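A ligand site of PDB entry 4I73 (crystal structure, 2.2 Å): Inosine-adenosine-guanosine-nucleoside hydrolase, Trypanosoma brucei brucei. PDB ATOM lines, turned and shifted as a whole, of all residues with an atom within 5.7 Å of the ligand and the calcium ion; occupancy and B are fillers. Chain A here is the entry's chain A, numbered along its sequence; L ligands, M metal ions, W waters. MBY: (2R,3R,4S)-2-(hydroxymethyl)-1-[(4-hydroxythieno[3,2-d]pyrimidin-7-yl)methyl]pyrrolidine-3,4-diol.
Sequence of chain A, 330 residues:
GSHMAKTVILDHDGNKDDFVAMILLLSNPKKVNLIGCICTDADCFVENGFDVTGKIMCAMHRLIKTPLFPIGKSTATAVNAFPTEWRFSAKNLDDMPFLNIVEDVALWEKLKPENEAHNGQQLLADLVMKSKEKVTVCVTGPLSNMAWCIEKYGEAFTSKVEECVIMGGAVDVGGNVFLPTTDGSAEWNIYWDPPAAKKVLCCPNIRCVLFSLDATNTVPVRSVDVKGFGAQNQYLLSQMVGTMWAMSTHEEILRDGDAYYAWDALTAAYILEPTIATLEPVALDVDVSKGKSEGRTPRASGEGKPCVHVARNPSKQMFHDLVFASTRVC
OD1 of Asp 17 lies close to O2' of the ligand, at 2.5 Å.
The guanidinium group (NH1) of Arg 255 sits at hydrogen-bond distance from an oxygen (O6) of the ligand, at 2.5 Å.
The side-chain carboxylate of Glu 187 lies within hydrogen-bond range of an oxygen (O5') of the ligand (2.5 Å).
A nitrogen (N4') of the ligand lies within salt-bridge range of the side-chain carboxylate of Asp 43.
ND2 of Asn 189 sits close to O3' of the ligand (3.3 Å).
The side-chain amide nitrogen of Asn 176 sits at hydrogen-bond distance from an oxygen (O5') of the ligand (3.4 Å).
The backbone carbonyl oxygen of Thr 140 sits close to the side-chain amide nitrogen of Asn 189 (3.4 Å).
N of Asp 43 lies close to OD2 of Asp 13 (3.1 Å).
The backbone NH (N) of Asp 264 is in hydrogen-bond range of the side-chain carboxylate (OD2) of Asp 17, 2.8 Å away.
The backbone carbonyl oxygen of Ala 259 lies within hydrogen-bond range of the guanidinium group of Arg 255, 3.1 Å away.
The side-chain carboxylate (OE2) of Glu 251 is in salt-bridge range of the guanidinium group (NE) of Arg 255.
OE2 of Glu 187 is in hydrogen-bond range of N of Asn 189, at 2.8 Å.
The backbone carbonyl oxygen of Met 167 lies within hydrogen-bond range of the side-chain amide nitrogen of Asn 189 (2.9 Å).
The side-chain hydroxyl (OH) of Tyr 260 sits at hydrogen-bond distance from the side-chain amide oxygen (OD1) of Asn 15.
Asn 15 touches the ligand (OD1 to C2, 3.999 Å).
CE1 of Phe 82 touches C7 of the ligand, at 3.4 Å.
Trp 86 touches the ligand (CZ3 to C5, 3.3 Å).
Met 167 touches the ligand (SD to O3', 3.9 Å).
Trp 188 touches the ligand.
Tyr 260 touches the ligand (CE1 to N1, 3.7 Å).
Trp 263 touches the ligand (CE3 to C2', 3.5 Å).
16 residues have an atom within 4 Å of the ligand: Asn 15, Asp 17, Asp 18, Asp 43, Phe 82, Trp 86, Thr 140, Met 167, Asn 176, Glu 187, Trp 188, Asn 189, Arg 255, Tyr 260, Trp 263 and Asp 264.
The nearest printed residue that does not touch the ligand is Asp 13 (4.3 Å).
Within 4 Å of the calcium ion: Asp 13, Asp 18, Thr 140 and Asp 264.
The calcium ion is bound by the backbone carbonyl oxygen (O) of Thr 140 (2.3 Å), the side-chain carboxylate (OD1) of Asp 13 (2.3 Å), the side-chain carboxylate (OD2) of Asp 264 (2.4 Å), an oxygen (O2') of the ligand (2.5 Å), the side-chain carboxylate (OD2) of Asp 18 (2.5 Å), the side-chain carboxylate (OD1) of Asp 18 (2.5 Å), an oxygen (O3') of the ligand (2.6 Å) and water W3 (2.7 Å).
Water W3 lies within hydrogen-bond range of the side-chain amide oxygen of Asn 189 (2.6 Å) and the side-chain carboxylate of Asp 13 (2.7 Å).
Water W1 bridges OD1 of Asn 15 (2.7 Å) and O of Trp 86 (3.3 Å).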
ATOM      1  N   HIS A  12     -12.844   4.849 -22.241  1.00  0.00           N
ATOM      2  CA  HIS A  12     -13.927   5.632 -22.849  1.00  0.00           C
ATOM      3  C   HIS A  12     -14.679   6.503 -21.863  1.00  0.00           C
ATOM      4  O   HIS A  12     -14.506   6.341 -20.622  1.00  0.00           O
ATOM      5  CB  HIS A  12     -14.925   4.726 -23.548  1.00  0.00           C
ATOM      6  CG  HIS A  12     -15.770   3.920 -22.631  1.00  0.00           C
ATOM      7  ND1 HIS A  12     -16.898   4.424 -22.041  1.00  0.00           N
ATOM      8  CD2 HIS A  12     -15.660   2.644 -22.239  1.00  0.00           C
ATOM      9  CE1 HIS A  12     -17.432   3.496 -21.255  1.00  0.00           C
ATOM     10  NE2 HIS A  12     -16.701   2.395 -21.370  1.00  0.00           N
ATOM     11  N   ASP A  13     -15.506   7.407 -22.388  1.00  0.00           N
ATOM     12  CA  ASP A  13     -16.286   8.231 -21.516  1.00  0.00           C
ATOM     13  C   ASP A  13     -17.788   8.153 -21.743  1.00  0.00           C
ATOM     14  O   ASP A  13     -18.500   9.143 -21.547  1.00  0.00           O
ATOM     15  CB  ASP A  13     -15.778   9.668 -21.568  1.00  0.00           C
ATOM     16  CG  ASP A  13     -16.039  10.330 -22.874  1.00  0.00           C
ATOM     17  OD1 ASP A  13     -16.264   9.625 -23.904  1.00  0.00           O
ATOM     18  OD2 ASP A  13     -15.975  11.598 -22.839  1.00  0.00           O
ATOM     19  N   GLY A  14     -18.261   6.996 -22.196  1.00  0.00           N
ATOM     20  CA  GLY A  14     -19.689   6.667 -22.080  1.00  0.00           C
ATOM     21  C   GLY A  14     -20.751   7.459 -22.837  1.00  0.00           C
ATOM     22  O   GLY A  14     -21.911   7.547 -22.396  1.00  0.00           O
ATOM     23  N   ASN A  15     -20.425   8.058 -23.963  1.00  0.00           N
ATOM     24  CA  ASN A  15     -21.497   8.573 -24.815  1.00  0.00           C
ATOM     25  C   ASN A  15     -21.876   7.484 -25.849  1.00  0.00           C
ATOM     26  O   ASN A  15     -21.366   6.383 -25.791  1.00  0.00           O
ATOM     27  CB  ASN A  15     -21.122   9.871 -25.470  1.00  0.00           C
ATOM     28  CG  ASN A  15     -22.280  10.831 -25.587  1.00  0.00           C
ATOM     29  OD1 ASN A  15     -23.015  10.860 -26.610  1.00  0.00           O
ATOM     30  ND2 ASN A  15     -22.498  11.624 -24.518  1.00  0.00           N
ATOM     31  N   ASP A  17     -21.499   6.991 -29.122  1.00  0.00           N
ATOM     32  CA  ASP A  17     -20.451   6.484 -29.978  1.00  0.00           C
ATOM     33  C   ASP A  17     -19.403   5.654 -29.189  1.00  0.00           C
ATOM     34  O   ASP A  17     -18.925   4.668 -29.722  1.00  0.00           O
ATOM     35  CB  ASP A  17     -19.803   7.600 -30.788  1.00  0.00           C
ATOM     36  CG  ASP A  17     -18.988   8.551 -29.948  1.00  0.00           C
ATOM     37  OD1 ASP A  17     -19.320   8.780 -28.757  1.00  0.00           O
ATOM     38  OD2 ASP A  17     -17.994   9.033 -30.501  1.00  0.00           O
ATOM     39  N   ASP A  18     -19.098   6.005 -27.939  1.00  0.00           N
ATOM     40  CA  ASP A  18     -18.147   5.203 -27.150  1.00  0.00           C
ATOM     41  C   ASP A  18     -18.651   3.770 -27.112  1.00  0.00           C
ATOM     42  O   ASP A  18     -17.887   2.843 -27.228  1.00  0.00           O
ATOM     43  CB  ASP A  18     -17.999   5.687 -25.716  1.00  0.00           C
ATOM     44  CG  ASP A  18     -17.370   7.058 -25.621  1.00  0.00           C
ATOM     45  OD1 ASP A  18     -16.136   7.144 -25.365  1.00  0.00           O
ATOM     46  OD2 ASP A  18     -18.120   8.056 -25.790  1.00  0.00           O
ATOM     47  N   ASP A  43     -18.026  12.709 -20.801  1.00  0.00           N
ATOM     48  CA  ASP A  43     -19.201  12.903 -21.653  1.00  0.00           C
ATOM     49  C   ASP A  43     -20.337  11.974 -21.216  1.00  0.00           C
ATOM     50  O   ASP A  43     -21.138  11.497 -22.060  1.00  0.00           O
ATOM     51  CB  ASP A  43     -18.879  12.634 -23.095  1.00  0.00           C
ATOM     52  CG  ASP A  43     -19.752  13.389 -24.057  1.00  0.00           C
ATOM     53  OD1 ASP A  43     -20.567  14.284 -23.693  1.00  0.00           O
ATOM     54  OD2 ASP A  43     -19.638  13.090 -25.235  1.00  0.00           O
ATOM     55  N   PHE A  82     -18.022  18.806 -19.640  1.00  0.00           N
ATOM     56  CA  PHE A  82     -18.930  18.674 -20.765  1.00  0.00           C
ATOM     57  C   PHE A  82     -20.325  19.269 -20.469  1.00  0.00           C
ATOM     58  O   PHE A  82     -20.788  19.279 -19.318  1.00  0.00           O
ATOM     59  CB  PHE A  82     -19.106  17.192 -21.157  1.00  0.00           C
ATOM     60  CG  PHE A  82     -18.020  16.651 -22.065  1.00  0.00           C
ATOM     61  CD1 PHE A  82     -18.111  16.815 -23.435  1.00  0.00           C
ATOM     62  CD2 PHE A  82     -16.980  15.910 -21.576  1.00  0.00           C
ATOM     63  CE1 PHE A  82     -17.167  16.304 -24.286  1.00  0.00           C
ATOM     64  CE2 PHE A  82     -16.016  15.387 -22.433  1.00  0.00           C
ATOM     65  CZ  PHE A  82     -16.136  15.563 -23.792  1.00  0.00           C
ATOM     66  N   TRP A  86     -25.436  16.612 -23.011  1.00  0.00           N
ATOM     67  CA  TRP A  86     -24.764  15.511 -23.670  1.00  0.00           C
ATOM     68  C   TRP A  86     -24.455  14.327 -22.738  1.00  0.00           C
ATOM     69  O   TRP A  86     -24.504  13.197 -23.183  1.00  0.00           O
ATOM     70  CB  TRP A  86     -23.442  15.970 -24.272  1.00  0.00           C
ATOM     71  CG  TRP A  86     -23.535  17.006 -25.333  1.00  0.00           C
ATOM     72  CD1 TRP A  86     -24.651  17.479 -25.907  1.00  0.00           C
ATOM     73  CD2 TRP A  86     -22.437  17.692 -25.960  1.00  0.00           C
ATOM     74  NE1 TRP A  86     -24.342  18.430 -26.851  1.00  0.00           N
ATOM     75  CE2 TRP A  86     -22.988  18.584 -26.902  1.00  0.00           C
ATOM     76  CE3 TRP A  86     -21.048  17.635 -25.816  1.00  0.00           C
ATOM     77  CZ2 TRP A  86     -22.203  19.415 -27.691  1.00  0.00           C
ATOM     78  CZ3 TRP A  86     -20.261  18.444 -26.603  1.00  0.00           C
ATOM     79  CH2 TRP A  86     -20.845  19.336 -27.523  1.00  0.00           C
ATOM     80  N   THR A 140     -11.229   6.730 -26.072  1.00  0.00           N
ATOM     81  CA  THR A 140     -12.282   7.443 -26.780  1.00  0.00           C
ATOM     82  C   THR A 140     -12.902   8.553 -25.897  1.00  0.00           C
ATOM     83  O   THR A 140     -13.896   9.207 -26.299  1.00  0.00           O
ATOM     84  CB  THR A 140     -13.334   6.479 -27.289  1.00  0.00           C
ATOM     85  OG1 THR A 140     -13.921   5.824 -26.177  1.00  0.00           O
ATOM     86  CG2 THR A 140     -12.705   5.458 -28.229  1.00  0.00           C
ATOM     87  N   GLY A 141     -12.326   8.726 -24.711  1.00  0.00           N
ATOM     88  CA  GLY A 141     -12.601   9.855 -23.885  1.00  0.00           C
ATOM     89  C   GLY A 141     -11.340  10.680 -23.789  1.00  0.00           C
ATOM     90  O   GLY A 141     -10.431  10.532 -24.594  1.00  0.00           O
ATOM     91  N   MET A 167      -9.214   9.069 -30.121  1.00  0.00           N
ATOM     92  CA  MET A 167     -10.131  10.018 -30.707  1.00  0.00           C
ATOM     93  C   MET A 167      -9.921  11.347 -29.995  1.00  0.00           C
ATOM     94  O   MET A 167     -10.106  11.459 -28.785  1.00  0.00           O
ATOM     95  CB  MET A 167     -11.579   9.549 -30.571  1.00  0.00           C
ATOM     96  CG  MET A 167     -12.513  10.262 -31.535  1.00  0.00           C
ATOM     97  SD  MET A 167     -12.826  11.919 -30.937  1.00  0.00           S
ATOM     98  CE  MET A 167     -12.398  12.871 -32.392  1.00  0.00           C
ATOM     99  N   ASN A 176     -14.584  21.651 -32.199  1.00  0.00           N
ATOM    100  CA  ASN A 176     -15.997  21.543 -31.874  1.00  0.00           C
ATOM    101  C   ASN A 176     -16.396  22.028 -30.469  1.00  0.00           C
ATOM    102  O   ASN A 176     -17.531  21.838 -30.033  1.00  0.00           O
ATOM    103  CB  ASN A 176     -16.520  20.144 -32.191  1.00  0.00           C
ATOM    104  CG  ASN A 176     -15.899  19.051 -31.327  1.00  0.00           C
ATOM    105  OD1 ASN A 176     -15.161  19.304 -30.368  1.00  0.00           O
ATOM    106  ND2 ASN A 176     -16.246  17.794 -31.664  1.00  0.00           N
ATOM    107  N   GLU A 187     -11.010  20.697 -29.891  1.00  0.00           N
ATOM    108  CA  GLU A 187     -11.891  19.522 -29.890  1.00  0.00           C
ATOM    109  C   GLU A 187     -12.071  19.074 -28.431  1.00  0.00           C
ATOM    110  O   GLU A 187     -11.172  19.222 -27.609  1.00  0.00           O
ATOM    111  CB  GLU A 187     -11.282  18.408 -30.754  1.00  0.00           C
ATOM    112  CG  GLU A 187     -12.092  17.101 -30.778  1.00  0.00           C
ATOM    113  CD  GLU A 187     -11.886  16.231 -29.521  1.00  0.00           C
ATOM    114  OE1 GLU A 187     -10.766  16.208 -28.968  1.00  0.00           O
ATOM    115  OE2 GLU A 187     -12.856  15.562 -29.100  1.00  0.00           O
ATOM    116  N   TRP A 188     -13.261  18.534 -28.140  1.00  0.00           N
ATOM    117  CA  TRP A 188     -13.763  18.389 -26.761  1.00  0.00           C
ATOM    118  C   TRP A 188     -12.981  17.454 -25.850  1.00  0.00           C
ATOM    119  O   TRP A 188     -12.847  17.758 -24.659  1.00  0.00           O
ATOM    120  CB  TRP A 188     -15.254  17.988 -26.759  1.00  0.00           C
ATOM    121  CG  TRP A 188     -16.170  19.124 -26.507  1.00  0.00           C
ATOM    122  CD1 TRP A 188     -16.936  19.797 -27.434  1.00  0.00           C
ATOM    123  CD2 TRP A 188     -16.374  19.798 -25.256  1.00  0.00           C
ATOM    124  NE1 TRP A 188     -17.595  20.847 -26.830  1.00  0.00           N
ATOM    125  CE2 TRP A 188     -17.294  20.843 -25.483  1.00  0.00           C
ATOM    126  CE3 TRP A 188     -15.918  19.568 -23.952  1.00  0.00           C
ATOM    127  CZ2 TRP A 188     -17.760  21.674 -24.463  1.00  0.00           C
ATOM    128  CZ3 TRP A 188     -16.375  20.398 -22.937  1.00  0.00           C
ATOM    129  CH2 TRP A 188     -17.263  21.460 -23.205  1.00  0.00           C
ATOM    130  N   ASN A 189     -12.512  16.301 -26.383  1.00  0.00           N
ATOM    131  CA  ASN A 189     -11.736  15.348 -25.590  1.00  0.00           C
ATOM    132  C   ASN A 189     -10.380  15.941 -25.119  1.00  0.00           C
ATOM    133  O   ASN A 189      -9.870  15.594 -24.064  1.00  0.00           O
ATOM    134  CB  ASN A 189     -11.441  14.029 -26.355  1.00  0.00           C
ATOM    135  CG  ASN A 189     -12.668  13.104 -26.491  1.00  0.00           C
ATOM    136  OD1 ASN A 189     -13.700  13.250 -25.820  1.00  0.00           O
ATOM    137  ND2 ASN A 189     -12.544  12.152 -27.397  1.00  0.00           N
ATOM    138  N   LEU A 213     -10.730  15.495 -35.724  1.00  0.00           N
ATOM    139  CA  LEU A 213     -11.906  15.900 -36.463  1.00  0.00           C
ATOM    140  C   LEU A 213     -11.707  15.860 -37.996  1.00  0.00           C
ATOM    141  O   LEU A 213     -12.680  15.678 -38.731  1.00  0.00           O
ATOM    142  CB  LEU A 213     -12.391  17.264 -35.986  1.00  0.00           C
ATOM    143  CG  LEU A 213     -12.834  17.297 -34.496  1.00  0.00           C
ATOM    144  CD1 LEU A 213     -13.388  18.693 -34.123  1.00  0.00           C
ATOM    145  CD2 LEU A 213     -13.851  16.142 -34.193  1.00  0.00           C
ATOM    146  N   GLU A 251     -29.121  15.611 -35.142  1.00  0.00           N
ATOM    147  CA  GLU A 251     -28.197  16.712 -34.770  1.00  0.00           C
ATOM    148  C   GLU A 251     -27.670  17.519 -35.969  1.00  0.00           C
ATOM    149  O   GLU A 251     -27.522  18.761 -35.862  1.00  0.00           O
ATOM    150  CB  GLU A 251     -27.033  16.204 -33.925  1.00  0.00           C
ATOM    151  CG  GLU A 251     -27.435  15.551 -32.606  1.00  0.00           C
ATOM    152  CD  GLU A 251     -27.901  16.539 -31.546  1.00  0.00           C
ATOM    153  OE1 GLU A 251     -28.113  16.142 -30.387  1.00  0.00           O
ATOM    154  OE2 GLU A 251     -28.026  17.751 -31.853  1.00  0.00           O
ATOM    155  N   ARG A 255     -28.495  21.408 -35.750  1.00  0.00           N
ATOM    156  CA  ARG A 255     -27.308  22.252 -35.494  1.00  0.00           C
ATOM    157  C   ARG A 255     -26.602  22.708 -36.792  1.00  0.00           C
ATOM    158  O   ARG A 255     -25.397  23.021 -36.793  1.00  0.00           O
ATOM    159  CB  ARG A 255     -26.341  21.539 -34.552  1.00  0.00           C
ATOM    160  CG  ARG A 255     -27.006  20.980 -33.285  1.00  0.00           C
ATOM    161  CD  ARG A 255     -25.987  20.425 -32.262  1.00  0.00           C
ATOM    162  NE  ARG A 255     -25.106  19.385 -32.820  1.00  0.00           N
ATOM    163  CZ  ARG A 255     -24.320  18.579 -32.100  1.00  0.00           C
ATOM    164  NH1 ARG A 255     -24.298  18.652 -30.776  1.00  0.00           N
ATOM    165  NH2 ARG A 255     -23.565  17.675 -32.720  1.00  0.00           N
ATOM    166  N   ASP A 258     -23.610  20.659 -38.079  1.00  0.00           N
ATOM    167  CA  ASP A 258     -22.754  20.177 -36.992  1.00  0.00           C
ATOM    168  C   ASP A 258     -23.304  18.845 -36.476  1.00  0.00           C
ATOM    169  O   ASP A 258     -23.983  18.783 -35.453  1.00  0.00           O
ATOM    170  CB  ASP A 258     -22.653  21.216 -35.870  1.00  0.00           C
ATOM    171  CG  ASP A 258     -21.824  20.729 -34.679  1.00  0.00           C
ATOM    172  OD1 ASP A 258     -20.776  20.043 -34.923  1.00  0.00           O
ATOM    173  OD2 ASP A 258     -22.223  21.030 -33.515  1.00  0.00           O
ATOM    174  N   ALA A 259     -23.021  17.785 -37.215  1.00  0.00           N
ATOM    175  CA  ALA A 259     -23.664  16.479 -37.020  1.00  0.00           C
ATOM    176  C   ALA A 259     -23.173  15.780 -35.730  1.00  0.00           C
ATOM    177  O   ALA A 259     -22.177  16.195 -35.117  1.00  0.00           O
ATOM    178  CB  ALA A 259     -23.434  15.568 -38.273  1.00  0.00           C
ATOM    179  N   TYR A 260     -23.945  14.773 -35.288  1.00  0.00           N
ATOM    180  CA  TYR A 260     -23.415  13.737 -34.416  1.00  0.00           C
ATOM    181  C   TYR A 260     -22.671  12.834 -35.398  1.00  0.00           C
ATOM    182  O   TYR A 260     -23.251  12.364 -36.361  1.00  0.00           O
ATOM    183  CB  TYR A 260     -24.500  12.948 -33.663  1.00  0.00           C
ATOM    184  CG  TYR A 260     -23.979  12.169 -32.438  1.00  0.00           C
ATOM    185  CD1 TYR A 260     -23.905  12.787 -31.167  1.00  0.00           C
ATOM    186  CD2 TYR A 260     -23.584  10.828 -32.542  1.00  0.00           C
ATOM    187  CE1 TYR A 260     -23.432  12.085 -30.031  1.00  0.00           C
ATOM    188  CE2 TYR A 260     -23.092  10.113 -31.412  1.00  0.00           C
ATOM    189  CZ  TYR A 260     -23.015  10.751 -30.172  1.00  0.00           C
ATOM    190  OH  TYR A 260     -22.564  10.031 -29.105  1.00  0.00           O
ATOM    191  N   TRP A 263     -17.680   9.341 -34.304  1.00  0.00           N
ATOM    192  CA  TRP A 263     -16.338   9.675 -33.879  1.00  0.00           C
ATOM    193  C   TRP A 263     -15.567   8.479 -33.335  1.00  0.00           C
ATOM    194  O   TRP A 263     -14.563   8.057 -33.948  1.00  0.00           O
ATOM    195  CB  TRP A 263     -16.359  10.741 -32.778  1.00  0.00           C
ATOM    196  CG  TRP A 263     -16.979  12.063 -33.053  1.00  0.00           C
ATOM    197  CD1 TRP A 263     -16.372  13.166 -33.651  1.00  0.00           C
ATOM    198  CD2 TRP A 263     -18.242  12.514 -32.560  1.00  0.00           C
ATOM    199  NE1 TRP A 263     -17.238  14.245 -33.595  1.00  0.00           N
ATOM    200  CE2 TRP A 263     -18.373  13.881 -32.926  1.00  0.00           C
ATOM    201  CE3 TRP A 263     -19.285  11.909 -31.848  1.00  0.00           C
ATOM    202  CZ2 TRP A 263     -19.513  14.629 -32.621  1.00  0.00           C
ATOM    203  CZ3 TRP A 263     -20.417  12.689 -31.548  1.00  0.00           C
ATOM    204  CH2 TRP A 263     -20.517  14.007 -31.942  1.00  0.00           C
ATOM    205  N   ASP A 264     -16.015   7.955 -32.211  1.00  0.00           N
ATOM    206  CA  ASP A 264     -15.294   6.921 -31.504  1.00  0.00           C
ATOM    207  C   ASP A 264     -15.394   5.593 -32.213  1.00  0.00           C
ATOM    208  O   ASP A 264     -14.539   4.725 -32.008  1.00  0.00           O
ATOM    209  CB  ASP A 264     -15.771   6.781 -30.050  1.00  0.00           C
ATOM    210  CG  ASP A 264     -15.623   8.080 -29.233  1.00  0.00           C
ATOM    211  OD1 ASP A 264     -14.831   8.938 -29.648  1.00  0.00           O
ATOM    212  OD2 ASP A 264     -16.297   8.251 -28.181  1.00  0.00           O
HETATM  213  O6  MBY L   1     -22.599  16.986 -30.054  1.00  0.00           O
HETATM  214  C6  MBY L   1     -22.013  16.266 -29.254  1.00  0.00           C
HETATM  215  N1  MBY L   1     -22.682  15.400 -28.454  1.00  0.00           N
HETATM  216  C2  MBY L   1     -22.041  14.626 -27.536  1.00  0.00           C
HETATM  217  N3  MBY L   1     -20.722  14.654 -27.425  1.00  0.00           N
HETATM  218  C4  MBY L   1     -19.958  15.457 -28.174  1.00  0.00           C
HETATM  219  C5  MBY L   1     -20.545  16.324 -29.153  1.00  0.00           C
HETATM  220  C9  MBY L   1     -18.467  15.621 -28.198  1.00  0.00           C
HETATM  221  C8  MBY L   1     -18.073  16.572 -29.122  1.00  0.00           C
HETATM  222  S7  MBY L   1     -19.409  17.244 -29.988  1.00  0.00           S
HETATM  223  C7  MBY L   1     -17.487  14.858 -27.310  1.00  0.00           C
HETATM  224  N4' MBY L   1     -17.208  13.459 -27.754  1.00  0.00           N
HETATM  225  C4' MBY L   1     -16.021  13.203 -28.650  1.00  0.00           C
HETATM  226  C5' MBY L   1     -15.959  14.112 -29.879  1.00  0.00           C
HETATM  227  O5' MBY L   1     -15.293  15.361 -29.567  1.00  0.00           O
HETATM  228  C3' MBY L   1     -16.215  11.753 -29.067  1.00  0.00           C
HETATM  229  O3' MBY L   1     -15.411  10.873 -28.250  1.00  0.00           O
HETATM  230  C2' MBY L   1     -17.714  11.446 -28.804  1.00  0.00           C
HETATM  231  O2' MBY L   1     -17.831  10.476 -27.768  1.00  0.00           O
HETATM  232  C1' MBY L   1     -18.345  12.710 -28.334  1.00  0.00           C
HETATM  233 CA    CA M   1     -16.141   9.543 -26.190  1.00  0.00          CA
HETATM  234  O   HOH W   1     -24.745  12.891 -26.463  1.00  0.00           O
HETATM  235  O   HOH W   2     -25.236  14.682 -28.383  1.00  0.00           O
HETATM  236  O   HOH W   3     -16.072  12.203 -25.497  1.00  0.00           O
